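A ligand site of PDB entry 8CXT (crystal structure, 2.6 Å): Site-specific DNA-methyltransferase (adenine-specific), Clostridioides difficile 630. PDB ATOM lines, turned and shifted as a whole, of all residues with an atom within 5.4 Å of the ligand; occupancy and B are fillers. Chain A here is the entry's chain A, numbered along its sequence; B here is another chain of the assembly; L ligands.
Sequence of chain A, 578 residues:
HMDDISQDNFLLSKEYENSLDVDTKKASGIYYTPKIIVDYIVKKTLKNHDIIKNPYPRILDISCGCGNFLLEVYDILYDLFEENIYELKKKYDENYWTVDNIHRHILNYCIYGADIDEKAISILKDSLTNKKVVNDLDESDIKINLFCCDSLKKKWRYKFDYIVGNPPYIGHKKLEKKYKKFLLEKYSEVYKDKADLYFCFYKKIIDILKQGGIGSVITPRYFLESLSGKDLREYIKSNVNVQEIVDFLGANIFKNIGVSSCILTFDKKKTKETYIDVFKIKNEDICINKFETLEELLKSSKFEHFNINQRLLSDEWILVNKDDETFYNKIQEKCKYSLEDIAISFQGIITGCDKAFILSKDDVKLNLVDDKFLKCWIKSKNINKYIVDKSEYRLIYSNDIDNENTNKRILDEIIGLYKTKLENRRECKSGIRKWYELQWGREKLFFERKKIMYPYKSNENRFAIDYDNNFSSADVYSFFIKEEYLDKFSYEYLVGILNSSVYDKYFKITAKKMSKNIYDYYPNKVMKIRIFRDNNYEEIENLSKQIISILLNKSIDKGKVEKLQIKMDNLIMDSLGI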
ATOM      1  N   GLY A  29      13.874 -23.182 -35.569  1.00  0.00           N
ATOM      2  CA  GLY A  29      13.430 -22.502 -34.371  1.00  0.00           C
ATOM      3  C   GLY A  29      12.418 -23.278 -33.549  1.00  0.00           C
ATOM      4  O   GLY A  29      11.893 -22.763 -32.549  1.00  0.00           O
ATOM      5  N   ILE A  30      12.120 -24.512 -33.956  1.00  0.00           N
ATOM      6  CA  ILE A  30      11.170 -25.376 -33.257  1.00  0.00           C
ATOM      7  C   ILE A  30      11.937 -26.579 -32.727  1.00  0.00           C
ATOM      8  O   ILE A  30      12.581 -27.309 -33.500  1.00  0.00           O
ATOM      9  CB  ILE A  30      10.021 -25.814 -34.169  1.00  0.00           C
ATOM     10  N   TYR A  31      11.854 -26.800 -31.418  1.00  0.00           N
ATOM     11  CA  TYR A  31      12.587 -27.855 -30.735  1.00  0.00           C
ATOM     12  C   TYR A  31      11.604 -28.867 -30.150  1.00  0.00           C
ATOM     13  O   TYR A  31      10.622 -28.476 -29.506  1.00  0.00           O
ATOM     14  CB  TYR A  31      13.472 -27.295 -29.620  1.00  0.00           C
ATOM     15  CG  TYR A  31      14.495 -26.273 -30.078  1.00  0.00           C
ATOM     16  CD1 TYR A  31      14.137 -24.938 -30.281  1.00  0.00           C
ATOM     17  CD2 TYR A  31      15.818 -26.637 -30.306  1.00  0.00           C
ATOM     18  CE1 TYR A  31      15.071 -24.004 -30.697  1.00  0.00           C
ATOM     19  CE2 TYR A  31      16.752 -25.704 -30.721  1.00  0.00           C
ATOM     20  CZ  TYR A  31      16.376 -24.393 -30.919  1.00  0.00           C
ATOM     21  OH  TYR A  31      17.304 -23.467 -31.330  1.00  0.00           O
ATOM     22  N   ILE A  62       2.182 -21.121 -24.421  1.00  0.00           N
ATOM     23  CA  ILE A  62       2.484 -19.898 -25.166  1.00  0.00           C
ATOM     24  C   ILE A  62       3.697 -20.096 -26.054  1.00  0.00           C
ATOM     25  O   ILE A  62       4.215 -19.137 -26.638  1.00  0.00           O
ATOM     26  CB  ILE A  62       2.690 -18.698 -24.225  1.00  0.00           C
ATOM     27  CG1 ILE A  62       3.670 -19.027 -23.099  1.00  0.00           C
ATOM     28  CG2 ILE A  62       1.363 -18.199 -23.675  1.00  0.00           C
ATOM     29  CD1 ILE A  62       3.947 -17.856 -22.188  1.00  0.00           C
ATOM     30  N   SER A  63       4.167 -21.336 -26.170  1.00  0.00           N
ATOM     31  CA  SER A  63       5.189 -21.708 -27.137  1.00  0.00           C
ATOM     32  C   SER A  63       4.845 -23.047 -27.765  1.00  0.00           C
ATOM     33  O   SER A  63       5.711 -23.909 -27.941  1.00  0.00           O
ATOM     34  CB  SER A  63       6.577 -21.754 -26.498  1.00  0.00           C
ATOM     35  OG  SER A  63       6.986 -20.463 -26.060  1.00  0.00           O
ATOM     36  N   CYS A  64       3.567 -23.226 -28.120  1.00  0.00           N
ATOM     37  CA  CYS A  64       3.051 -24.561 -28.437  1.00  0.00           C
ATOM     38  C   CYS A  64       3.762 -25.194 -29.627  1.00  0.00           C
ATOM     39  O   CYS A  64       3.903 -26.422 -29.668  1.00  0.00           O
ATOM     40  CB  CYS A  64       1.547 -24.494 -28.693  1.00  0.00           C
ATOM     41  SG  CYS A  64       1.084 -23.401 -30.052  1.00  0.00           S
ATOM     42  N   GLY A  65       4.226 -24.393 -30.577  1.00  0.00           N
ATOM     43  CA  GLY A  65       4.891 -24.960 -31.739  1.00  0.00           C
ATOM     44  C   GLY A  65       3.963 -25.882 -32.505  1.00  0.00           C
ATOM     45  O   GLY A  65       2.852 -25.496 -32.903  1.00  0.00           O
ATOM     46  N   ALA A 114      -0.338 -20.469 -28.321  1.00  0.00           N
ATOM     47  CA  ALA A 114       0.181 -19.302 -29.006  1.00  0.00           C
ATOM     48  C   ALA A 114       1.592 -19.579 -29.509  1.00  0.00           C
ATOM     49  O   ALA A 114       2.408 -20.169 -28.795  1.00  0.00           O
ATOM     50  CB  ALA A 114       0.196 -18.067 -28.098  1.00  0.00           C
ATOM     51  N   ASP A 115       1.871 -19.161 -30.745  1.00  0.00           N
ATOM     52  CA  ASP A 115       3.210 -19.317 -31.309  1.00  0.00           C
ATOM     53  C   ASP A 115       3.389 -18.298 -32.421  1.00  0.00           C
ATOM     54  O   ASP A 115       2.423 -17.791 -32.998  1.00  0.00           O
ATOM     55  CB  ASP A 115       3.432 -20.743 -31.826  1.00  0.00           C
ATOM     56  CG  ASP A 115       4.909 -21.116 -31.867  1.00  0.00           C
ATOM     57  OD1 ASP A 115       5.673 -20.455 -32.612  1.00  0.00           O
ATOM     58  OD2 ASP A 115       5.306 -22.056 -31.148  1.00  0.00           O
ATOM     59  N   ILE A 116       4.661 -18.013 -32.735  1.00  0.00           N
ATOM     60  CA  ILE A 116       4.994 -16.997 -33.738  1.00  0.00           C
ATOM     61  C   ILE A 116       5.031 -17.570 -35.152  1.00  0.00           C
ATOM     62  O   ILE A 116       5.053 -16.797 -36.119  1.00  0.00           O
ATOM     63  CB  ILE A 116       6.329 -16.325 -33.370  1.00  0.00           C
ATOM     64  CG1 ILE A 116       6.556 -15.028 -34.154  1.00  0.00           C
ATOM     65  CG2 ILE A 116       7.486 -17.290 -33.579  1.00  0.00           C
ATOM     66  CD1 ILE A 116       5.583 -13.925 -33.816  1.00  0.00           C
ATOM     67  N   ASP A 117       5.020 -18.893 -35.305  1.00  0.00           N
ATOM     68  CA  ASP A 117       5.196 -19.540 -36.595  1.00  0.00           C
ATOM     69  C   ASP A 117       3.835 -19.949 -37.153  1.00  0.00           C
ATOM     70  O   ASP A 117       3.099 -20.718 -36.515  1.00  0.00           O
ATOM     71  CB  ASP A 117       6.101 -20.763 -36.462  1.00  0.00           C
ATOM     72  CG  ASP A 117       6.331 -21.480 -37.777  1.00  0.00           C
ATOM     73  OD1 ASP A 117       6.116 -20.867 -38.844  1.00  0.00           O
ATOM     74  OD2 ASP A 117       6.738 -22.660 -37.748  1.00  0.00           O
ATOM     75  N   CYS A 149       1.142 -15.099 -32.924  1.00  0.00           N
ATOM     76  CA  CYS A 149       1.517 -13.799 -32.393  1.00  0.00           C
ATOM     77  C   CYS A 149       2.823 -13.922 -31.622  1.00  0.00           C
ATOM     78  O   CYS A 149       3.408 -15.005 -31.508  1.00  0.00           O
ATOM     79  CB  CYS A 149       0.408 -13.238 -31.498  1.00  0.00           C
ATOM     80  SG  CYS A 149       0.237 -14.120 -29.917  1.00  0.00           S
ATOM     81  N   ASP A 150       3.276 -12.783 -31.100  1.00  0.00           N
ATOM     82  CA  ASP A 150       4.388 -12.713 -30.155  1.00  0.00           C
ATOM     83  C   ASP A 150       3.802 -12.711 -28.758  1.00  0.00           C
ATOM     84  O   ASP A 150       3.160 -11.735 -28.349  1.00  0.00           O
ATOM     85  CB  ASP A 150       5.230 -11.463 -30.415  1.00  0.00           C
ATOM     86  CG  ASP A 150       6.463 -11.365 -29.530  1.00  0.00           C
ATOM     87  OD1 ASP A 150       6.495 -11.971 -28.439  1.00  0.00           O
ATOM     88  OD2 ASP A 150       7.412 -10.657 -29.932  1.00  0.00           O
ATOM     89  N   SER A 151       4.016 -13.801 -28.012  1.00  0.00           N
ATOM     90  CA  SER A 151       3.370 -13.956 -26.711  1.00  0.00           C
ATOM     91  C   SER A 151       3.790 -12.869 -25.730  1.00  0.00           C
ATOM     92  O   SER A 151       3.030 -12.579 -24.785  1.00  0.00           O
ATOM     93  CB  SER A 151       3.702 -15.332 -26.131  1.00  0.00           C
ATOM     94  OG  SER A 151       3.198 -16.361 -26.954  1.00  0.00           O
ATOM     95  N   LEU A 152       4.952 -12.251 -25.912  1.00  0.00           N
ATOM     96  CA  LEU A 152       5.410 -11.202 -25.016  1.00  0.00           C
ATOM     97  C   LEU A 152       4.812  -9.843 -25.329  1.00  0.00           C
ATOM     98  O   LEU A 152       4.986  -8.913 -24.537  1.00  0.00           O
ATOM     99  CB  LEU A 152       6.939 -11.112 -25.047  1.00  0.00           C
ATOM    100  CG  LEU A 152       7.666 -12.337 -24.513  1.00  0.00           C
ATOM    101  CD1 LEU A 152       9.157 -12.099 -24.502  1.00  0.00           C
ATOM    102  CD2 LEU A 152       7.168 -12.687 -23.111  1.00  0.00           C
ATOM    103  N   ASN A 166       7.442 -25.329 -23.280  1.00  0.00           N
ATOM    104  CA  ASN A 166       8.890 -25.159 -23.416  1.00  0.00           C
ATOM    105  C   ASN A 166       9.142 -23.831 -24.124  1.00  0.00           C
ATOM    106  O   ASN A 166       9.002 -23.752 -25.363  1.00  0.00           O
ATOM    107  CB  ASN A 166       9.493 -26.327 -24.192  1.00  0.00           C
ATOM    108  CG  ASN A 166      10.992 -26.206 -24.368  1.00  0.00           C
ATOM    109  OD1 ASN A 166      11.656 -25.430 -23.675  1.00  0.00           O
ATOM    110  ND2 ASN A 166      11.546 -26.967 -25.301  1.00  0.00           N
ATOM    111  N   PRO A 167       9.522 -22.784 -23.398  1.00  0.00           N
ATOM    112  CA  PRO A 167       9.669 -21.459 -24.015  1.00  0.00           C
ATOM    113  C   PRO A 167      10.948 -21.372 -24.839  1.00  0.00           C
ATOM    114  O   PRO A 167      11.803 -22.264 -24.772  1.00  0.00           O
ATOM    115  CB  PRO A 167       9.738 -20.518 -22.796  1.00  0.00           C
ATOM    116  CG  PRO A 167      10.379 -21.365 -21.743  1.00  0.00           C
ATOM    117  CD  PRO A 167       9.850 -22.770 -21.960  1.00  0.00           C
ATOM    118  N   PRO A 168      11.103 -20.320 -25.642  1.00  0.00           N
ATOM    119  CA  PRO A 168      12.359 -20.136 -26.388  1.00  0.00           C
ATOM    120  C   PRO A 168      13.474 -19.597 -25.511  1.00  0.00           C
ATOM    121  O   PRO A 168      13.247 -18.731 -24.650  1.00  0.00           O
ATOM    122  CB  PRO A 168      11.972 -19.133 -27.474  1.00  0.00           C
ATOM    123  CG  PRO A 168      10.881 -18.340 -26.858  1.00  0.00           C
ATOM    124  CD  PRO A 168      10.088 -19.323 -26.028  1.00  0.00           C
ATOM    125  N   ILE A 170      16.870 -17.545 -25.825  1.00  0.00           N
ATOM    126  CA  ILE A 170      17.740 -16.718 -26.656  1.00  0.00           C
ATOM    127  C   ILE A 170      18.575 -15.816 -25.763  1.00  0.00           C
ATOM    128  O   ILE A 170      18.025 -15.020 -24.991  1.00  0.00           O
ATOM    129  CB  ILE A 170      16.959 -15.878 -27.688  1.00  0.00           C
ATOM    130  CG1 ILE A 170      15.976 -16.752 -28.461  1.00  0.00           C
ATOM    131  CG2 ILE A 170      17.925 -15.217 -28.660  1.00  0.00           C
ATOM    132  CD1 ILE A 170      15.228 -16.014 -29.544  1.00  0.00           C
ATOM    133  N   LEU A 175      20.021 -12.040 -29.792  1.00  0.00           N
ATOM    134  CA  LEU A 175      18.764 -11.317 -29.739  1.00  0.00           C
ATOM    135  C   LEU A 175      18.914  -9.986 -30.471  1.00  0.00           C
ATOM    136  O   LEU A 175      19.884  -9.260 -30.231  1.00  0.00           O
ATOM    137  CB  LEU A 175      18.334 -11.092 -28.285  1.00  0.00           C
ATOM    138  CG  LEU A 175      16.844 -10.997 -27.957  1.00  0.00           C
ATOM    139  CD1 LEU A 175      16.071 -12.148 -28.573  1.00  0.00           C
ATOM    140  CD2 LEU A 175      16.652 -10.994 -26.448  1.00  0.00           C
ATOM    141  N   TYR A 179      14.458  -5.462 -30.381  1.00  0.00           N
ATOM    142  CA  TYR A 179      13.658  -6.282 -29.470  1.00  0.00           C
ATOM    143  C   TYR A 179      14.223  -6.229 -28.054  1.00  0.00           C
ATOM    144  O   TYR A 179      13.467  -6.263 -27.072  1.00  0.00           O
ATOM    145  CB  TYR A 179      13.597  -7.710 -29.978  1.00  0.00           C
ATOM    146  CG  TYR A 179      12.467  -8.504 -29.375  1.00  0.00           C
ATOM    147  CD1 TYR A 179      11.196  -8.475 -29.930  1.00  0.00           C
ATOM    148  CD2 TYR A 179      12.660  -9.280 -28.238  1.00  0.00           C
ATOM    149  CE1 TYR A 179      10.154  -9.191 -29.385  1.00  0.00           C
ATOM    150  CE2 TYR A 179      11.626  -9.995 -27.681  1.00  0.00           C
ATOM    151  CZ  TYR A 179      10.366  -9.943 -28.254  1.00  0.00           C
ATOM    152  OH  TYR A 179       9.332 -10.664 -27.705  1.00  0.00           O
ATOM    153  N   LEU A 197      15.759 -14.299 -22.700  1.00  0.00           N
ATOM    154  CA  LEU A 197      14.363 -14.125 -23.073  1.00  0.00           C
ATOM    155  C   LEU A 197      13.433 -14.991 -22.225  1.00  0.00           C
ATOM    156  O   LEU A 197      12.308 -14.574 -21.880  1.00  0.00           O
ATOM    157  CB  LEU A 197      14.208 -14.454 -24.560  1.00  0.00           C
ATOM    158  CG  LEU A 197      12.869 -14.334 -25.290  1.00  0.00           C
ATOM    159  CD1 LEU A 197      12.477 -12.880 -25.443  1.00  0.00           C
ATOM    160  CD2 LEU A 197      12.964 -15.011 -26.642  1.00  0.00           C
ATOM    161  N   PHE A 201       9.607 -14.865 -20.426  1.00  0.00           N
ATOM    162  CA  PHE A 201       8.534 -15.860 -20.505  1.00  0.00           C
ATOM    163  C   PHE A 201       8.095 -16.326 -19.119  1.00  0.00           C
ATOM    164  O   PHE A 201       6.900 -16.524 -18.883  1.00  0.00           O
ATOM    165  CB  PHE A 201       8.958 -17.038 -21.380  1.00  0.00           C
ATOM    166  CG  PHE A 201       8.632 -16.844 -22.833  1.00  0.00           C
ATOM    167  CD1 PHE A 201       9.445 -16.074 -23.645  1.00  0.00           C
ATOM    168  CD2 PHE A 201       7.486 -17.419 -23.375  1.00  0.00           C
ATOM    169  CE1 PHE A 201       9.137 -15.889 -24.981  1.00  0.00           C
ATOM    170  CE2 PHE A 201       7.178 -17.233 -24.711  1.00  0.00           C
ATOM    171  CZ  PHE A 201       7.999 -16.463 -25.512  1.00  0.00           C
ATOM    172  P    DA B   8      23.236 -20.251 -25.787  1.00  0.00           P
ATOM    173  OP1  DA B   8      23.767 -20.084 -27.156  1.00  0.00           O
ATOM    174  OP2  DA B   8      22.370 -19.207 -25.199  1.00  0.00           O
ATOM    175  O5'  DA B   8      22.471 -21.646 -25.683  1.00  0.00           O
ATOM    176  C5'  DA B   8      21.144 -21.779 -26.145  1.00  0.00           C
ATOM    177  C4'  DA B   8      20.887 -23.196 -26.595  1.00  0.00           C
ATOM    178  O4'  DA B   8      19.540 -23.586 -26.264  1.00  0.00           O
ATOM    179  C3'  DA B   8      21.051 -23.433 -28.094  1.00  0.00           C
ATOM    180  O3'  DA B   8      21.676 -24.682 -28.317  1.00  0.00           O
ATOM    181  C2'  DA B   8      19.609 -23.431 -28.589  1.00  0.00           C
ATOM    182  C1'  DA B   8      18.911 -24.095 -27.423  1.00  0.00           C
ATOM    183  N9   DA B   8      17.487 -23.782 -27.329  1.00  0.00           N
ATOM    184  C8   DA B   8      16.892 -22.572 -27.522  1.00  0.00           C
ATOM    185  N7   DA B   8      15.582 -22.590 -27.364  1.00  0.00           N
ATOM    186  C5   DA B   8      15.309 -23.911 -27.030  1.00  0.00           C
ATOM    187  C6   DA B   8      14.112 -24.584 -26.734  1.00  0.00           C
ATOM    188  N6   DA B   8      12.920 -23.989 -26.726  1.00  0.00           N
ATOM    189  N1   DA B   8      14.191 -25.903 -26.449  1.00  0.00           N
ATOM    190  C2   DA B   8      15.390 -26.491 -26.462  1.00  0.00           C
ATOM    191  N3   DA B   8      16.581 -25.963 -26.727  1.00  0.00           N
ATOM    192  C4   DA B   8      16.468 -24.653 -27.005  1.00  0.00           C
HETATM  193  N1  LIG L   1       9.670 -16.806 -29.677  1.00  0.00           N
HETATM  194  C1  LIG L   1       7.575 -17.712 -29.695  1.00  0.00           C
HETATM  195  C2  LIG L   1       5.673 -16.686 -29.228  1.00  0.00           C
HETATM  196  N2  LIG L   1       6.248 -17.836 -29.596  1.00  0.00           N
HETATM  197  C3  LIG L   1       7.591 -15.412 -29.076  1.00  0.00           C
HETATM  198  O1  LIG L   1       8.295 -20.395 -32.724  1.00  0.00           O
HETATM  199  C4  LIG L   1       8.979 -20.663 -31.498  1.00  0.00           C
HETATM  200  C5  LIG L   1       9.708 -18.069 -30.024  1.00  0.00           C
HETATM  201  C6  LIG L   1       8.314 -16.567 -29.469  1.00  0.00           C
HETATM  202  N3  LIG L   1       6.254 -15.508 -28.972  1.00  0.00           N
HETATM  203  C7  LIG L   1       8.208 -20.094 -30.322  1.00  0.00           C
HETATM  204  C8  LIG L   1      10.042 -22.780 -28.908  1.00  0.00           C
HETATM  205  O2  LIG L   1       8.605 -20.858 -29.199  1.00  0.00           O
HETATM  206  C9  LIG L   1       8.848 -22.207 -29.650  1.00  0.00           C
HETATM  207  N4  LIG L   1       8.157 -14.235 -28.757  1.00  0.00           N
HETATM  208  N5  LIG L   1       8.479 -18.689 -30.037  1.00  0.00           N
HETATM  209  C10 LIG L   1       8.985 -22.168 -31.175  1.00  0.00           C
HETATM  210  O3  LIG L   1       7.906 -22.859 -31.807  1.00  0.00           O
HETATM  211  C11 LIG L   1       9.590 -13.991 -28.749  1.00  0.00           C
HETATM  212  C12 LIG L   1      10.087 -13.334 -30.015  1.00  0.00           C
HETATM  213  C13 LIG L   1      11.425 -12.954 -30.140  1.00  0.00           C
HETATM  214  C14 LIG L   1      11.879 -12.352 -31.304  1.00  0.00           C
HETATM  215  C15 LIG L   1      11.008 -12.111 -32.344  1.00  0.00           C
HETATM  216  C16 LIG L   1       9.682 -12.478 -32.229  1.00  0.00           C
HETATM  217  C17 LIG L   1       9.228 -13.086 -31.074  1.00  0.00           C
HETATM  218  O4  LIG L   1      11.269 -22.314 -29.463  1.00  0.00           O
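OD1 of Asp 115 sits at hydrogen-bond distance from O1 of the ligand, 2.6 Å away.
OD1 of Asp 150 sits at hydrogen-bond distance from N4 of the ligand, 2.8 Å away.
The backbone NH (N) of Ser 151 is in hydrogen-bond range of a nitrogen (N3) of the ligand (3.0 Å).
The backbone carbonyl oxygen (O) of Gly 29 is in hydrogen-bond range of an oxygen (O4) of the ligand.
Tyr 31 touches the ligand.
Ile 62 touches the ligand.
Ser 63 touches the ligand.
Gly 65 touches the ligand.
Ile 116 touches the ligand.
Cys 149 touches the ligand.
Asn 166 touches the ligand.
Pro 168 touches the ligand.
OH of Tyr 179 touches C11 of the ligand, at 3.5 Å.
CZ of Phe 201 touches C3 of the ligand (3.7 Å).
DA 8 of chain B touches the ligand (N6 to O4, 3.6 Å).
15 residues have an atom within 4 Å of the ligand: Gly 29, Tyr 31, Ile 62, Ser 63, Gly 65, Asp 115, Ile 116, Cys 149, Asp 150, Ser 151, Asn 166, Pro 168, Tyr 179, Phe 201 and DA 8 of chain B.
Along chain A the residues within 4 Å of the ligand span positions 29 to 201.
O of Asp 115 lies within hydrogen-bond range of N of Cys 149 (3.0 Å).
The side-chain carboxylate (OD2) of Asp 115 is in hydrogen-bond range of the backbone NH (N) of Gly 65 (2.6 Å).
The side-chain carboxylate (OD1) of Asp 115 sits at hydrogen-bond distance from the backbone NH (N) of Asp 117, at 3.2 Å.
OD2 of Asp 150 sits at hydrogen-bond distance from OH of Tyr 179 (2.9 Å).
N of Leu 152 sits at hydrogen-bond distance from OD1 of Asp 150, at 3.0 Å.
The side-chain hydroxyl of Ser 151 is in hydrogen-bond range of the backbone carbonyl oxygen of Ile 62.
N of Ile 116 sits close to O of Cys 149 (3.5 Å).
N of Ser 63 is in hydrogen-bond range of O of Ala 114, at 3.4 Å.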
